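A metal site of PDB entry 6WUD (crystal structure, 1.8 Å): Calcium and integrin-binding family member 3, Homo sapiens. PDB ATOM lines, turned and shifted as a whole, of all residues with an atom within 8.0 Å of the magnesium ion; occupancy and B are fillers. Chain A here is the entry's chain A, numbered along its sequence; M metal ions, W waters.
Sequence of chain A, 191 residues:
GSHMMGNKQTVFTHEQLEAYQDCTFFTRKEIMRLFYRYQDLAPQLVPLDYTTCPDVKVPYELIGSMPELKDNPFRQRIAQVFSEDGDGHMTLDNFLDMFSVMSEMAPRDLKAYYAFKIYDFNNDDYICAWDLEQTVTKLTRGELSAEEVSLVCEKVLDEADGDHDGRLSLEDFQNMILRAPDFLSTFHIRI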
ATOM      1  N   TYR A 126     -13.777  -2.846  10.454  1.00  0.00           N
ATOM      2  CA  TYR A 126     -13.948  -1.420  10.657  1.00  0.00           C
ATOM      3  C   TYR A 126     -14.192  -0.766   9.309  1.00  0.00           C
ATOM      4  O   TYR A 126     -13.745  -1.281   8.284  1.00  0.00           O
ATOM      5  CB  TYR A 126     -12.728  -0.745  11.309  1.00  0.00           C
ATOM      6  CG  TYR A 126     -12.529  -1.168  12.735  1.00  0.00           C
ATOM      7  CD1 TYR A 126     -13.185  -0.499  13.767  1.00  0.00           C
ATOM      8  CD2 TYR A 126     -11.689  -2.218  13.051  1.00  0.00           C
ATOM      9  CE1 TYR A 126     -13.030  -0.876  15.062  1.00  0.00           C
ATOM     10  CE2 TYR A 126     -11.533  -2.604  14.349  1.00  0.00           C
ATOM     11  CZ  TYR A 126     -12.204  -1.924  15.352  1.00  0.00           C
ATOM     12  OH  TYR A 126     -12.049  -2.300  16.648  1.00  0.00           O
ATOM     13  N   ILE A 127     -14.875   0.376   9.304  1.00  0.00           N
ATOM     14  CA  ILE A 127     -14.987   1.217   8.112  1.00  0.00           C
ATOM     15  C   ILE A 127     -14.201   2.489   8.393  1.00  0.00           C
ATOM     16  O   ILE A 127     -14.588   3.319   9.235  1.00  0.00           O
ATOM     17  CB  ILE A 127     -16.437   1.523   7.744  1.00  0.00           C
ATOM     18  CG1 ILE A 127     -17.112   0.230   7.279  1.00  0.00           C
ATOM     19  CG2 ILE A 127     -16.511   2.536   6.605  1.00  0.00           C
ATOM     20  CD1 ILE A 127     -18.606   0.388   7.045  1.00  0.00           C
ATOM     21  N   LEU A 157     -17.177  10.449   9.219  1.00  0.00           N
ATOM     22  CA  LEU A 157     -16.507  10.100  10.474  1.00  0.00           C
ATOM     23  C   LEU A 157     -16.894  11.049  11.603  1.00  0.00           C
ATOM     24  O   LEU A 157     -17.116  10.614  12.743  1.00  0.00           O
ATOM     25  CB  LEU A 157     -15.001  10.083  10.255  1.00  0.00           C
ATOM     26  CG  LEU A 157     -14.476   8.934   9.395  1.00  0.00           C
ATOM     27  CD1 LEU A 157     -12.965   9.098   9.152  1.00  0.00           C
ATOM     28  CD2 LEU A 157     -14.782   7.596  10.046  1.00  0.00           C
ATOM     29  N   ALA A 160     -20.527   9.964  12.587  1.00  0.00           N
ATOM     30  CA  ALA A 160     -20.871   8.612  12.981  1.00  0.00           C
ATOM     31  C   ALA A 160     -19.834   7.913  13.850  1.00  0.00           C
ATOM     32  O   ALA A 160     -20.153   6.852  14.409  1.00  0.00           O
ATOM     33  CB  ALA A 160     -21.131   7.757  11.728  1.00  0.00           C
ATOM     34  N   ASP A 161     -18.621   8.465  13.988  1.00  0.00           N
ATOM     35  CA  ASP A 161     -17.571   7.761  14.743  1.00  0.00           C
ATOM     36  C   ASP A 161     -17.791   8.020  16.237  1.00  0.00           C
ATOM     37  O   ASP A 161     -17.189   8.906  16.846  1.00  0.00           O
ATOM     38  CB  ASP A 161     -16.177   8.202  14.331  1.00  0.00           C
ATOM     39  CG  ASP A 161     -15.057   7.488  15.143  1.00  0.00           C
ATOM     40  OD1 ASP A 161     -15.294   6.403  15.691  1.00  0.00           O
ATOM     41  OD2 ASP A 161     -13.944   8.020  15.199  1.00  0.00           O
ATOM     42  N   GLY A 162     -18.651   7.188  16.840  1.00  0.00           N
ATOM     43  CA  GLY A 162     -19.125   7.455  18.184  1.00  0.00           C
ATOM     44  C   GLY A 162     -18.072   7.280  19.252  1.00  0.00           C
ATOM     45  O   GLY A 162     -18.026   8.051  20.205  1.00  0.00           O
ATOM     46  N   ASP A 163     -17.236   6.250  19.135  1.00  0.00           N
ATOM     47  CA  ASP A 163     -16.197   6.027  20.133  1.00  0.00           C
ATOM     48  C   ASP A 163     -14.923   6.799  19.818  1.00  0.00           C
ATOM     49  O   ASP A 163     -13.895   6.571  20.459  1.00  0.00           O
ATOM     50  CB  ASP A 163     -15.896   4.518  20.300  1.00  0.00           C
ATOM     51  CG  ASP A 163     -15.833   3.778  18.990  1.00  0.00           C
ATOM     52  OD1 ASP A 163     -16.033   2.538  19.003  1.00  0.00           O
ATOM     53  OD2 ASP A 163     -15.574   4.438  17.946  1.00  0.00           O
ATOM     54  N   HIS A 164     -14.980   7.696  18.836  1.00  0.00           N
ATOM     55  CA  HIS A 164     -13.912   8.652  18.566  1.00  0.00           C
ATOM     56  C   HIS A 164     -12.558   7.961  18.454  1.00  0.00           C
ATOM     57  O   HIS A 164     -11.589   8.356  19.090  1.00  0.00           O
ATOM     58  CB  HIS A 164     -13.900   9.758  19.644  1.00  0.00           C
ATOM     59  CG  HIS A 164     -15.012  10.755  19.495  1.00  0.00           C
ATOM     60  ND1 HIS A 164     -16.224  10.618  20.142  1.00  0.00           N
ATOM     61  CD2 HIS A 164     -15.125  11.861  18.721  1.00  0.00           C
ATOM     62  CE1 HIS A 164     -17.030  11.610  19.784  1.00  0.00           C
ATOM     63  NE2 HIS A 164     -16.388  12.376  18.920  1.00  0.00           N
ATOM     64  N   ASP A 165     -12.470   6.948  17.594  1.00  0.00           N
ATOM     65  CA  ASP A 165     -11.198   6.307  17.295  1.00  0.00           C
ATOM     66  C   ASP A 165     -10.741   6.513  15.860  1.00  0.00           C
ATOM     67  O   ASP A 165      -9.700   5.957  15.468  1.00  0.00           O
ATOM     68  CB  ASP A 165     -11.285   4.806  17.590  1.00  0.00           C
ATOM     69  CG  ASP A 165     -12.298   4.119  16.709  1.00  0.00           C
ATOM     70  OD1 ASP A 165     -13.033   4.837  15.990  1.00  0.00           O
ATOM     71  OD2 ASP A 165     -12.345   2.873  16.709  1.00  0.00           O
ATOM     72  N   GLY A 166     -11.464   7.295  15.058  1.00  0.00           N
ATOM     73  CA  GLY A 166     -11.094   7.543  13.672  1.00  0.00           C
ATOM     74  C   GLY A 166     -11.700   6.599  12.644  1.00  0.00           C
ATOM     75  O   GLY A 166     -11.320   6.640  11.464  1.00  0.00           O
ATOM     76  N   ARG A 167     -12.635   5.751  13.043  1.00  0.00           N
ATOM     77  CA  ARG A 167     -13.135   4.697  12.158  1.00  0.00           C
ATOM     78  C   ARG A 167     -14.427   4.156  12.753  1.00  0.00           C
ATOM     79  O   ARG A 167     -14.682   4.296  13.938  1.00  0.00           O
ATOM     80  CB  ARG A 167     -12.120   3.582  11.988  1.00  0.00           C
ATOM     81  CG  ARG A 167     -11.779   2.911  13.264  1.00  0.00           C
ATOM     82  CD  ARG A 167     -10.501   2.101  13.162  1.00  0.00           C
ATOM     83  NE  ARG A 167     -10.206   1.490  14.454  1.00  0.00           N
ATOM     84  CZ  ARG A 167      -9.439   0.420  14.633  1.00  0.00           C
ATOM     85  NH1 ARG A 167      -8.867  -0.195  13.605  1.00  0.00           N
ATOM     86  NH2 ARG A 167      -9.252  -0.030  15.868  1.00  0.00           N
ATOM     87  N   LEU A 168     -15.227   3.513  11.912  1.00  0.00           N
ATOM     88  CA  LEU A 168     -16.551   3.057  12.275  1.00  0.00           C
ATOM     89  C   LEU A 168     -16.476   1.583  12.650  1.00  0.00           C
ATOM     90  O   LEU A 168     -16.170   0.734  11.807  1.00  0.00           O
ATOM     91  CB  LEU A 168     -17.563   3.284  11.146  1.00  0.00           C
ATOM     92  CG  LEU A 168     -17.716   4.682  10.578  1.00  0.00           C
ATOM     93  CD1 LEU A 168     -18.837   4.765   9.549  1.00  0.00           C
ATOM     94  CD2 LEU A 168     -17.927   5.740  11.689  1.00  0.00           C
ATOM     95  N   SER A 169     -16.719   1.298  13.914  1.00  0.00           N
ATOM     96  CA  SER A 169     -16.969  -0.063  14.352  1.00  0.00           C
ATOM     97  C   SER A 169     -18.379  -0.468  13.927  1.00  0.00           C
ATOM     98  O   SER A 169     -19.201   0.354  13.512  1.00  0.00           O
ATOM     99  CB  SER A 169     -16.832  -0.162  15.864  1.00  0.00           C
ATOM    100  OG  SER A 169     -17.837   0.675  16.426  1.00  0.00           O
ATOM    101  N   LEU A 170     -18.665  -1.764  14.051  1.00  0.00           N
ATOM    102  CA  LEU A 170     -20.032  -2.216  13.799  1.00  0.00           C
ATOM    103  C   LEU A 170     -21.010  -1.446  14.672  1.00  0.00           C
ATOM    104  O   LEU A 170     -22.106  -1.088  14.218  1.00  0.00           O
ATOM    105  CB  LEU A 170     -20.156  -3.714  14.038  1.00  0.00           C
ATOM    106  CG  LEU A 170     -21.577  -4.273  13.930  1.00  0.00           C
ATOM    107  CD1 LEU A 170     -22.122  -4.002  12.549  1.00  0.00           C
ATOM    108  CD2 LEU A 170     -21.573  -5.762  14.231  1.00  0.00           C
ATOM    109  N   GLU A 171     -20.647  -1.227  15.937  1.00  0.00           N
ATOM    110  CA  GLU A 171     -21.525  -0.488  16.850  1.00  0.00           C
ATOM    111  C   GLU A 171     -21.736   0.949  16.384  1.00  0.00           C
ATOM    112  O   GLU A 171     -22.878   1.428  16.373  1.00  0.00           O
ATOM    113  CB  GLU A 171     -20.954  -0.542  18.260  1.00  0.00           C
ATOM    114  CG  GLU A 171     -20.333  -1.874  18.669  1.00  0.00           C
ATOM    115  CD  GLU A 171     -18.875  -2.057  18.210  1.00  0.00           C
ATOM    116  OE1 GLU A 171     -18.613  -2.963  17.407  1.00  0.00           O
ATOM    117  OE2 GLU A 171     -17.990  -1.294  18.648  1.00  0.00           O
ATOM    118  N   ASP A 172     -20.676   1.569  15.879  1.00  0.00           N
ATOM    119  CA  ASP A 172     -20.777   2.910  15.351  1.00  0.00           C
ATOM    120  C   ASP A 172     -21.736   2.925  14.175  1.00  0.00           C
ATOM    121  O   ASP A 172     -22.604   3.794  14.067  1.00  0.00           O
ATOM    122  CB  ASP A 172     -19.426   3.354  14.795  1.00  0.00           C
ATOM    123  CG  ASP A 172     -18.473   3.805  15.886  1.00  0.00           C
ATOM    124  OD1 ASP A 172     -18.953   4.148  16.988  1.00  0.00           O
ATOM    125  OD2 ASP A 172     -17.252   3.822  15.642  1.00  0.00           O
ATOM    126  N   PHE A 173     -21.585   1.936  13.298  1.00  0.00           N
ATOM    127  CA  PHE A 173     -22.369   1.867  12.078  1.00  0.00           C
ATOM    128  C   PHE A 173     -23.842   1.594  12.367  1.00  0.00           C
ATOM    129  O   PHE A 173     -24.735   2.262  11.820  1.00  0.00           O
ATOM    130  CB  PHE A 173     -21.769   0.779  11.177  1.00  0.00           C
ATOM    131  CG  PHE A 173     -22.433   0.653   9.837  1.00  0.00           C
ATOM    132  CD1 PHE A 173     -22.054   1.470   8.789  1.00  0.00           C
ATOM    133  CD2 PHE A 173     -23.444  -0.299   9.620  1.00  0.00           C
ATOM    134  CE1 PHE A 173     -22.653   1.363   7.542  1.00  0.00           C
ATOM    135  CE2 PHE A 173     -24.038  -0.420   8.399  1.00  0.00           C
ATOM    136  CZ  PHE A 173     -23.639   0.418   7.343  1.00  0.00           C
HETATM  137 MG    MG M   1     -15.233   4.544  16.064  1.00  0.00          MG
HETATM  138  O   HOH W   1     -14.656   2.601  16.099  1.00  0.00           O
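The side-chain carboxylate of Asp 161 lies close to the backbone NH of His 164, 3.4 Å away.
The backbone NH (N) of Gly 162 sits at hydrogen-bond distance from the side-chain carboxylate (OD1) of Asp 172 (3.1 Å).
N of Asp 172 lies within hydrogen-bond range of OG of Ser 169, 3.0 Å away.
The side-chain carboxylate (OD2) of Asp 161 lies within hydrogen-bond range of the backbone NH (N) of Gly 166.
The magnesium ion is bound by the side-chain carboxylate of Asp 161, the side-chain carboxylate of Asp 163, water W1, the side-chain carboxylate of Asp 172, the backbone carbonyl oxygen of Arg 167 and the side-chain carboxylate of Asp 165.
Water W1 lies within hydrogen-bond range of the side-chain carboxylate (OD2) of Asp 165, the side-chain carboxylate (OD1) of Asp 163 and the backbone NH (N) of Ser 169.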
